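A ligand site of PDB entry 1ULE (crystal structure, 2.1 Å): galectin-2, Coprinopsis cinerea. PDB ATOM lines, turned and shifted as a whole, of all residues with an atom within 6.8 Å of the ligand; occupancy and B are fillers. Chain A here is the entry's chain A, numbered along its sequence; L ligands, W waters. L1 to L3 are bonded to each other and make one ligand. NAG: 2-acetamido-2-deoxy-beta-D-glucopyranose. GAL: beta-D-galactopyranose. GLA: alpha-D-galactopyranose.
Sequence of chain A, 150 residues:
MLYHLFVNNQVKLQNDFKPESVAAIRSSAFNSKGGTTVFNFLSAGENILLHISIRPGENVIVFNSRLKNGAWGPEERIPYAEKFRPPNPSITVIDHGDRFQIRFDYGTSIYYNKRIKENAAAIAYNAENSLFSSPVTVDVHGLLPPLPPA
Merely in contact with the ligand: Ser 53 (3.7 Å) and Val 38 (3.8 Å).
Hydrophobic or aromatic side chains that line the ligand: Val 38, His 51 and Trp 72.
Of the 20 residues printed, 8 come within 4 Å of the ligand.
Along chain A the residues within 4 Å of the ligand span positions 38 to 77.
The guanidinium group (NE) of Arg 55 is in hydrogen-bond range of the side-chain hydroxyl (OG) of Ser 53.
The guanidinium group of Arg 55 is in salt-bridge range of the side-chain carboxylate of Glu 58 (3.3 Å).
The side-chain amide nitrogen of Asn 64 is in hydrogen-bond range of the backbone carbonyl oxygen of Gly 73 (2.8 Å).
OE1 of Glu 75 is in salt-bridge range of NH2 of Arg 77 (2.7 Å).
N of Asn 126 sits at hydrogen-bond distance from O of Val 38, 2.8 Å away.
The guanidinium group (NH1) of Arg 77 is in salt-bridge range of the side-chain carboxylate (OE2) of Glu 58.
O of Pro 74 sits close to OD1 of Asn 64 (3.5 Å).
The backbone NH (N) of Ser 53 lies within hydrogen-bond range of the backbone carbonyl oxygen (O) of Val 62 (2.7 Å).
Water W10 lies within hydrogen-bond range of O4 of GLA L3 and NH2 of Arg 66.
Water W8 lies within hydrogen-bond range of an oxygen (O7) of NAG L1 (2.6 Å) and the side-chain carboxylate (OE1) of Glu 75 (2.7 Å).
Water W9 lies within hydrogen-bond range of N2 of NAG L1 (2.6 Å), OE2 of Glu 58 (2.7 Å) and NH2 of Arg 77 (3.3 Å).
Water W2 bridges OG of Ser 53 and O4 of GAL L2.
Water W4 lies within hydrogen-bond range of O2 of GLA L3 (3.0 Å) and ND2 of Asn 126 (3.3 Å).
The guanidinium group of Arg 55 sits at hydrogen-bond distance from an oxygen (O3) of NAG L1 (2.8 Å).
An oxygen (O3) of NAG L1 lies close to the guanidinium group (NH2) of Arg 77, 3.1 Å away.
The side-chain amide nitrogen (ND2) of Asn 64 is in hydrogen-bond range of an oxygen (O6) of GAL L2 (2.9 Å).
An oxygen (O6) of GLA L3 is in hydrogen-bond range of the indole nitrogen (NE1) of Trp 72, 3.1 Å away.
NE2 of His 51 is in hydrogen-bond range of O4 of GAL L2 (2.7 Å).
An oxygen (O6) of GAL L2 sits at hydrogen-bond distance from the side-chain carboxylate (OE2) of Glu 75 (2.6 Å).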
ATOM      1  N   THR A  36      12.665  32.192  -6.924  1.00  0.00           N
ATOM      2  CA  THR A  36      12.825  30.982  -7.710  1.00  0.00           C
ATOM      3  C   THR A  36      13.630  31.277  -8.970  1.00  0.00           C
ATOM      4  O   THR A  36      13.369  32.227  -9.704  1.00  0.00           O
ATOM      5  CB  THR A  36      11.439  30.396  -8.081  1.00  0.00           C
ATOM      6  OG1 THR A  36      10.812  29.920  -6.890  1.00  0.00           O
ATOM      7  CG2 THR A  36      11.577  29.252  -9.074  1.00  0.00           C
ATOM      8  N   VAL A  38      15.312  29.442 -12.441  1.00  0.00           N
ATOM      9  CA  VAL A  38      15.227  28.295 -13.330  1.00  0.00           C
ATOM     10  C   VAL A  38      16.274  28.238 -14.443  1.00  0.00           C
ATOM     11  O   VAL A  38      16.659  29.259 -14.997  1.00  0.00           O
ATOM     12  CB  VAL A  38      13.818  28.260 -14.001  1.00  0.00           C
ATOM     13  CG1 VAL A  38      13.783  27.205 -15.091  1.00  0.00           C
ATOM     14  CG2 VAL A  38      12.754  27.985 -12.950  1.00  0.00           C
ATOM     15  N   ASN A  40      16.932  25.749 -17.919  1.00  0.00           N
ATOM     16  CA  ASN A  40      16.375  24.704 -18.780  1.00  0.00           C
ATOM     17  C   ASN A  40      17.335  24.322 -19.881  1.00  0.00           C
ATOM     18  O   ASN A  40      17.996  25.178 -20.453  1.00  0.00           O
ATOM     19  CB  ASN A  40      15.092  25.170 -19.500  1.00  0.00           C
ATOM     20  CG  ASN A  40      13.912  25.370 -18.561  1.00  0.00           C
ATOM     21  OD1 ASN A  40      13.704  24.591 -17.637  1.00  0.00           O
ATOM     22  ND2 ASN A  40      13.122  26.401 -18.826  1.00  0.00           N
ATOM     23  N   HIS A  51      14.681  20.473 -16.667  1.00  0.00           N
ATOM     24  CA  HIS A  51      14.196  21.677 -16.013  1.00  0.00           C
ATOM     25  C   HIS A  51      14.705  21.639 -14.572  1.00  0.00           C
ATOM     26  O   HIS A  51      14.483  20.665 -13.847  1.00  0.00           O
ATOM     27  CB  HIS A  51      12.667  21.660 -16.042  1.00  0.00           C
ATOM     28  CG  HIS A  51      12.015  22.743 -15.228  1.00  0.00           C
ATOM     29  ND1 HIS A  51      12.034  24.063 -15.594  1.00  0.00           N
ATOM     30  CD2 HIS A  51      11.279  22.676 -14.093  1.00  0.00           C
ATOM     31  CE1 HIS A  51      11.333  24.771 -14.726  1.00  0.00           C
ATOM     32  NE2 HIS A  51      10.860  23.942 -13.798  1.00  0.00           N
ATOM     33  N   ILE A  52      15.429  22.682 -14.164  1.00  0.00           N
ATOM     34  CA  ILE A  52      15.958  22.781 -12.817  1.00  0.00           C
ATOM     35  C   ILE A  52      15.350  24.028 -12.171  1.00  0.00           C
ATOM     36  O   ILE A  52      15.751  25.145 -12.501  1.00  0.00           O
ATOM     37  CB  ILE A  52      17.498  22.926 -12.810  1.00  0.00           C
ATOM     38  CG1 ILE A  52      18.146  21.775 -13.579  1.00  0.00           C
ATOM     39  CG2 ILE A  52      18.016  22.923 -11.375  1.00  0.00           C
ATOM     40  CD1 ILE A  52      19.649  21.917 -13.745  1.00  0.00           C
ATOM     41  N   SER A  53      14.407  23.812 -11.256  1.00  0.00           N
ATOM     42  CA  SER A  53      13.722  24.906 -10.570  1.00  0.00           C
ATOM     43  C   SER A  53      14.224  25.053  -9.136  1.00  0.00           C
ATOM     44  O   SER A  53      13.881  24.266  -8.259  1.00  0.00           O
ATOM     45  CB  SER A  53      12.203  24.643 -10.546  1.00  0.00           C
ATOM     46  OG  SER A  53      11.507  25.750 -10.018  1.00  0.00           O
ATOM     47  N   ARG A  55      14.069  26.739  -5.773  1.00  0.00           N
ATOM     48  CA  ARG A  55      13.116  27.523  -4.974  1.00  0.00           C
ATOM     49  C   ARG A  55      13.555  27.686  -3.522  1.00  0.00           C
ATOM     50  O   ARG A  55      13.305  26.815  -2.689  1.00  0.00           O
ATOM     51  CB  ARG A  55      11.748  26.842  -5.020  1.00  0.00           C
ATOM     52  CG  ARG A  55      11.321  26.416  -6.418  1.00  0.00           C
ATOM     53  CD  ARG A  55      10.032  25.621  -6.401  1.00  0.00           C
ATOM     54  NE  ARG A  55       9.739  25.029  -7.711  1.00  0.00           N
ATOM     55  CZ  ARG A  55       8.719  24.216  -7.946  1.00  0.00           C
ATOM     56  NH1 ARG A  55       7.873  23.898  -6.978  1.00  0.00           N
ATOM     57  NH2 ARG A  55       8.542  23.714  -9.166  1.00  0.00           N
ATOM     58  N   GLU A  58      10.595  27.720  -0.891  1.00  0.00           N
ATOM     59  CA  GLU A  58       9.952  26.435  -0.635  1.00  0.00           C
ATOM     60  C   GLU A  58      11.019  25.451  -0.150  1.00  0.00           C
ATOM     61  O   GLU A  58      10.722  24.276   0.101  1.00  0.00           O
ATOM     62  CB  GLU A  58       9.305  25.946  -1.941  1.00  0.00           C
ATOM     63  CG  GLU A  58       8.262  24.845  -1.800  1.00  0.00           C
ATOM     64  CD  GLU A  58       7.701  24.399  -3.156  1.00  0.00           C
ATOM     65  OE1 GLU A  58       7.515  25.267  -4.036  1.00  0.00           O
ATOM     66  OE2 GLU A  58       7.436  23.191  -3.322  1.00  0.00           O
ATOM     67  N   VAL A  62      13.583  21.578  -7.801  1.00  0.00           N
ATOM     68  CA  VAL A  62      12.781  20.621  -8.544  1.00  0.00           C
ATOM     69  C   VAL A  62      13.307  20.321  -9.945  1.00  0.00           C
ATOM     70  O   VAL A  62      13.711  21.223 -10.674  1.00  0.00           O
ATOM     71  CB  VAL A  62      11.322  21.122  -8.631  1.00  0.00           C
ATOM     72  CG1 VAL A  62      10.448  20.078  -9.320  1.00  0.00           C
ATOM     73  CG2 VAL A  62      10.801  21.434  -7.237  1.00  0.00           C
ATOM     74  N   PHE A  63      13.277  19.042 -10.313  1.00  0.00           N
ATOM     75  CA  PHE A  63      13.724  18.592 -11.623  1.00  0.00           C
ATOM     76  C   PHE A  63      12.535  17.979 -12.363  1.00  0.00           C
ATOM     77  O   PHE A  63      11.751  17.245 -11.764  1.00  0.00           O
ATOM     78  CB  PHE A  63      14.838  17.557 -11.499  1.00  0.00           C
ATOM     79  CG  PHE A  63      16.046  18.040 -10.735  1.00  0.00           C
ATOM     80  CD1 PHE A  63      16.075  17.999  -9.340  1.00  0.00           C
ATOM     81  CD2 PHE A  63      17.139  18.579 -11.415  1.00  0.00           C
ATOM     82  CE1 PHE A  63      17.182  18.472  -8.635  1.00  0.00           C
ATOM     83  CE2 PHE A  63      18.245  19.052 -10.711  1.00  0.00           C
ATOM     84  CZ  PHE A  63      18.267  19.004  -9.317  1.00  0.00           C
ATOM     85  N   ASN A  64      12.411  18.266 -13.652  1.00  0.00           N
ATOM     86  CA  ASN A  64      11.306  17.746 -14.458  1.00  0.00           C
ATOM     87  C   ASN A  64      11.636  17.924 -15.943  1.00  0.00           C
ATOM     88  O   ASN A  64      12.712  18.405 -16.302  1.00  0.00           O
ATOM     89  CB  ASN A  64      10.012  18.502 -14.127  1.00  0.00           C
ATOM     90  CG  ASN A  64       8.763  17.637 -14.274  1.00  0.00           C
ATOM     91  OD1 ASN A  64       8.724  16.716 -15.088  1.00  0.00           O
ATOM     92  ND2 ASN A  64       7.735  17.962 -13.500  1.00  0.00           N
ATOM     93  N   SER A  65      10.680  17.542 -16.797  1.00  0.00           N
ATOM     94  CA  SER A  65      10.831  17.677 -18.253  1.00  0.00           C
ATOM     95  C   SER A  65       9.435  17.870 -18.837  1.00  0.00           C
ATOM     96  O   SER A  65       8.434  17.620 -18.167  1.00  0.00           O
ATOM     97  CB  SER A  65      11.422  16.395 -18.866  1.00  0.00           C
ATOM     98  OG  SER A  65      12.670  16.037 -18.298  1.00  0.00           O
ATOM     99  N   ARG A  66       9.362  18.328 -20.086  1.00  0.00           N
ATOM    100  CA  ARG A  66       8.080  18.483 -20.754  1.00  0.00           C
ATOM    101  C   ARG A  66       8.277  18.879 -22.210  1.00  0.00           C
ATOM    102  O   ARG A  66       9.224  19.591 -22.546  1.00  0.00           O
ATOM    103  CB  ARG A  66       7.182  19.512 -20.041  1.00  0.00           C
ATOM    104  CG  ARG A  66       7.383  20.963 -20.445  1.00  0.00           C
ATOM    105  CD  ARG A  66       6.267  21.847 -19.874  1.00  0.00           C
ATOM    106  NE  ARG A  66       6.523  23.275 -20.091  1.00  0.00           N
ATOM    107  CZ  ARG A  66       6.304  23.914 -21.233  1.00  0.00           C
ATOM    108  NH1 ARG A  66       5.820  23.269 -22.274  1.00  0.00           N
ATOM    109  NH2 ARG A  66       6.595  25.201 -21.341  1.00  0.00           N
ATOM    110  N   TRP A  72       3.926  19.032 -17.728  1.00  0.00           N
ATOM    111  CA  TRP A  72       5.030  18.627 -16.877  1.00  0.00           C
ATOM    112  C   TRP A  72       4.830  17.157 -16.509  1.00  0.00           C
ATOM    113  O   TRP A  72       3.709  16.676 -16.451  1.00  0.00           O
ATOM    114  CB  TRP A  72       5.059  19.454 -15.584  1.00  0.00           C
ATOM    115  CG  TRP A  72       5.496  20.881 -15.786  1.00  0.00           C
ATOM    116  CD1 TRP A  72       4.732  22.004 -15.640  1.00  0.00           C
ATOM    117  CD2 TRP A  72       6.783  21.325 -16.222  1.00  0.00           C
ATOM    118  NE1 TRP A  72       5.471  23.122 -15.966  1.00  0.00           N
ATOM    119  CE2 TRP A  72       6.732  22.734 -16.331  1.00  0.00           C
ATOM    120  CE3 TRP A  72       7.987  20.676 -16.545  1.00  0.00           C
ATOM    121  CZ2 TRP A  72       7.824  23.505 -16.736  1.00  0.00           C
ATOM    122  CZ3 TRP A  72       9.082  21.430 -16.950  1.00  0.00           C
ATOM    123  CH2 TRP A  72       8.989  22.834 -17.048  1.00  0.00           C
ATOM    124  N   GLY A  73       5.928  16.443 -16.257  1.00  0.00           N
ATOM    125  CA  GLY A  73       5.813  15.054 -15.866  1.00  0.00           C
ATOM    126  C   GLY A  73       5.893  15.015 -14.353  1.00  0.00           C
ATOM    127  O   GLY A  73       5.676  16.030 -13.704  1.00  0.00           O
ATOM    128  N   PRO A  74       6.181  13.851 -13.745  1.00  0.00           N
ATOM    129  CA  PRO A  74       6.284  13.759 -12.283  1.00  0.00           C
ATOM    130  C   PRO A  74       7.559  14.460 -11.807  1.00  0.00           C
ATOM    131  O   PRO A  74       8.577  14.418 -12.502  1.00  0.00           O
ATOM    132  CB  PRO A  74       6.301  12.256 -12.027  1.00  0.00           C
ATOM    133  CG  PRO A  74       6.949  11.711 -13.275  1.00  0.00           C
ATOM    134  CD  PRO A  74       6.273  12.515 -14.356  1.00  0.00           C
ATOM    135  N   GLU A  75       7.508  15.100 -10.651  1.00  0.00           N
ATOM    136  CA  GLU A  75       8.659  15.829 -10.132  1.00  0.00           C
ATOM    137  C   GLU A  75       9.639  14.968  -9.350  1.00  0.00           C
ATOM    138  O   GLU A  75       9.284  13.953  -8.766  1.00  0.00           O
ATOM    139  CB  GLU A  75       8.205  16.976  -9.232  1.00  0.00           C
ATOM    140  CG  GLU A  75       7.257  17.982  -9.874  1.00  0.00           C
ATOM    141  CD  GLU A  75       6.942  19.158  -8.964  1.00  0.00           C
ATOM    142  OE1 GLU A  75       6.851  18.953  -7.739  1.00  0.00           O
ATOM    143  OE2 GLU A  75       6.774  20.289  -9.483  1.00  0.00           O
ATOM    144  N   GLU A  76      10.899  15.398  -9.374  1.00  0.00           N
ATOM    145  CA  GLU A  76      11.971  14.750  -8.638  1.00  0.00           C
ATOM    146  C   GLU A  76      12.536  15.904  -7.822  1.00  0.00           C
ATOM    147  O   GLU A  76      12.947  16.928  -8.382  1.00  0.00           O
ATOM    148  CB  GLU A  76      12.987  14.122  -9.592  1.00  0.00           C
ATOM    149  CG  GLU A  76      12.401  12.885 -10.294  1.00  0.00           C
ATOM    150  CD  GLU A  76      13.325  12.241 -11.326  1.00  0.00           C
ATOM    151  OE1 GLU A  76      14.516  12.031 -11.015  1.00  0.00           O
ATOM    152  OE2 GLU A  76      12.853  11.931 -12.445  1.00  0.00           O
ATOM    153  N   ARG A  77      12.534  15.756  -6.507  1.00  0.00           N
ATOM    154  CA  ARG A  77      12.968  16.817  -5.609  1.00  0.00           C
ATOM    155  C   ARG A  77      14.128  16.519  -4.664  1.00  0.00           C
ATOM    156  O   ARG A  77      14.450  15.369  -4.386  1.00  0.00           O
ATOM    157  CB  ARG A  77      11.791  17.274  -4.757  1.00  0.00           C
ATOM    158  CG  ARG A  77      10.586  17.764  -5.536  1.00  0.00           C
ATOM    159  CD  ARG A  77       9.387  17.960  -4.618  1.00  0.00           C
ATOM    160  NE  ARG A  77       8.318  18.701  -5.275  1.00  0.00           N
ATOM    161  CZ  ARG A  77       7.871  19.889  -4.860  1.00  0.00           C
ATOM    162  NH1 ARG A  77       8.394  20.454  -3.784  1.00  0.00           N
ATOM    163  NH2 ARG A  77       6.914  20.502  -5.533  1.00  0.00           N
ATOM    164  N   ASN A 126      15.848  31.593 -16.413  1.00  0.00           N
ATOM    165  CA  ASN A 126      14.708  32.463 -16.121  1.00  0.00           C
ATOM    166  C   ASN A 126      14.552  32.796 -14.634  1.00  0.00           C
ATOM    167  O   ASN A 126      14.767  31.947 -13.776  1.00  0.00           O
ATOM    168  CB  ASN A 126      13.401  31.828 -16.607  1.00  0.00           C
ATOM    169  CG  ASN A 126      13.448  31.472 -18.074  1.00  0.00           C
ATOM    170  OD1 ASN A 126      13.704  32.326 -18.919  1.00  0.00           O
ATOM    171  ND2 ASN A 126      13.198  30.200 -18.381  1.00  0.00           N
HETATM  172  C1  NAG L   1       2.077  21.999  -7.677  1.00  0.00           C
HETATM  173  C2  NAG L   1       3.520  21.531  -7.492  1.00  0.00           C
HETATM  174  C3  NAG L   1       4.450  22.613  -8.034  1.00  0.00           C
HETATM  175  C4  NAG L   1       4.108  22.909  -9.491  1.00  0.00           C
HETATM  176  C5  NAG L   1       2.610  23.257  -9.622  1.00  0.00           C
HETATM  177  C6  NAG L   1       2.150  23.465 -11.060  1.00  0.00           C
HETATM  178  C7  NAG L   1       3.793  20.028  -5.620  1.00  0.00           C
HETATM  179  C8  NAG L   1       4.226  19.829  -4.168  1.00  0.00           C
HETATM  180  N2  NAG L   1       3.794  21.276  -6.085  1.00  0.00           N
HETATM  181  O1  NAG L   1       1.218  21.014  -7.219  1.00  0.00           O
HETATM  182  O3  NAG L   1       5.808  22.200  -7.934  1.00  0.00           O
HETATM  183  O4  NAG L   1       4.898  24.021  -9.935  1.00  0.00           O
HETATM  184  O5  NAG L   1       1.811  22.198  -9.072  1.00  0.00           O
HETATM  185  O6  NAG L   1       2.500  22.362 -11.889  1.00  0.00           O
HETATM  186  O7  NAG L   1       3.482  19.058  -6.306  1.00  0.00           O
HETATM  187  C1  GAL L   2       5.444  23.912 -11.202  1.00  0.00           C
HETATM  188  C2  GAL L   2       6.011  25.256 -11.592  1.00  0.00           C
HETATM  189  C3  GAL L   2       6.672  25.143 -12.957  1.00  0.00           C
HETATM  190  C4  GAL L   2       7.734  24.035 -12.957  1.00  0.00           C
HETATM  191  C5  GAL L   2       7.094  22.724 -12.464  1.00  0.00           C
HETATM  192  C6  GAL L   2       8.098  21.607 -12.319  1.00  0.00           C
HETATM  193  O2  GAL L   2       4.954  26.209 -11.638  1.00  0.00           O
HETATM  194  O3  GAL L   2       7.281  26.401 -13.303  1.00  0.00           O
HETATM  195  O4  GAL L   2       8.815  24.391 -12.110  1.00  0.00           O
HETATM  196  O5  GAL L   2       6.480  22.926 -11.168  1.00  0.00           O
HETATM  197  O6  GAL L   2       7.445  20.391 -11.957  1.00  0.00           O
HETATM  198  C1  GLA L   3       7.474  26.616 -14.675  1.00  0.00           C
HETATM  199  C2  GLA L   3       7.978  28.038 -14.901  1.00  0.00           C
HETATM  200  C3  GLA L   3       6.866  29.035 -14.588  1.00  0.00           C
HETATM  201  C4  GLA L   3       5.625  28.708 -15.417  1.00  0.00           C
HETATM  202  C5  GLA L   3       5.198  27.256 -15.160  1.00  0.00           C
HETATM  203  C6  GLA L   3       4.025  26.824 -16.025  1.00  0.00           C
HETATM  204  O2  GLA L   3       9.088  28.287 -14.042  1.00  0.00           O
HETATM  205  O3  GLA L   3       7.313  30.347 -14.888  1.00  0.00           O
HETATM  206  O4  GLA L   3       5.916  28.881 -16.795  1.00  0.00           O
HETATM  207  O5  GLA L   3       6.299  26.364 -15.441  1.00  0.00           O
HETATM  208  O6  GLA L   3       3.593  25.512 -15.670  1.00  0.00           O
HETATM  209  O   HOH W   1       2.557  26.538 -13.184  1.00  0.00           O
HETATM  210  O   HOH W   2       9.573  26.959 -11.331  1.00  0.00           O
HETATM  211  O   HOH W   3       3.610  30.443 -17.983  1.00  0.00           O
HETATM  212  O   HOH W   4      10.881  29.447 -16.176  1.00  0.00           O
HETATM  213  O   HOH W   5       4.445  20.165 -12.125  1.00  0.00           O
HETATM  214  O   HOH W   6       8.573  30.745 -17.778  1.00  0.00           O
HETATM  215  O   HOH W   7       0.239  19.425  -9.502  1.00  0.00           O
HETATM  216  O   HOH W   8       5.185  17.111  -6.739  1.00  0.00           O
HETATM  217  O   HOH W   9       5.077  23.093  -4.691  1.00  0.00           O
HETATM  218  O   HOH W  10       6.423  27.716 -19.080  1.00  0.00           O
HETATM  219  O   HOH W  11      10.489  30.774 -13.950  1.00  0.00           O
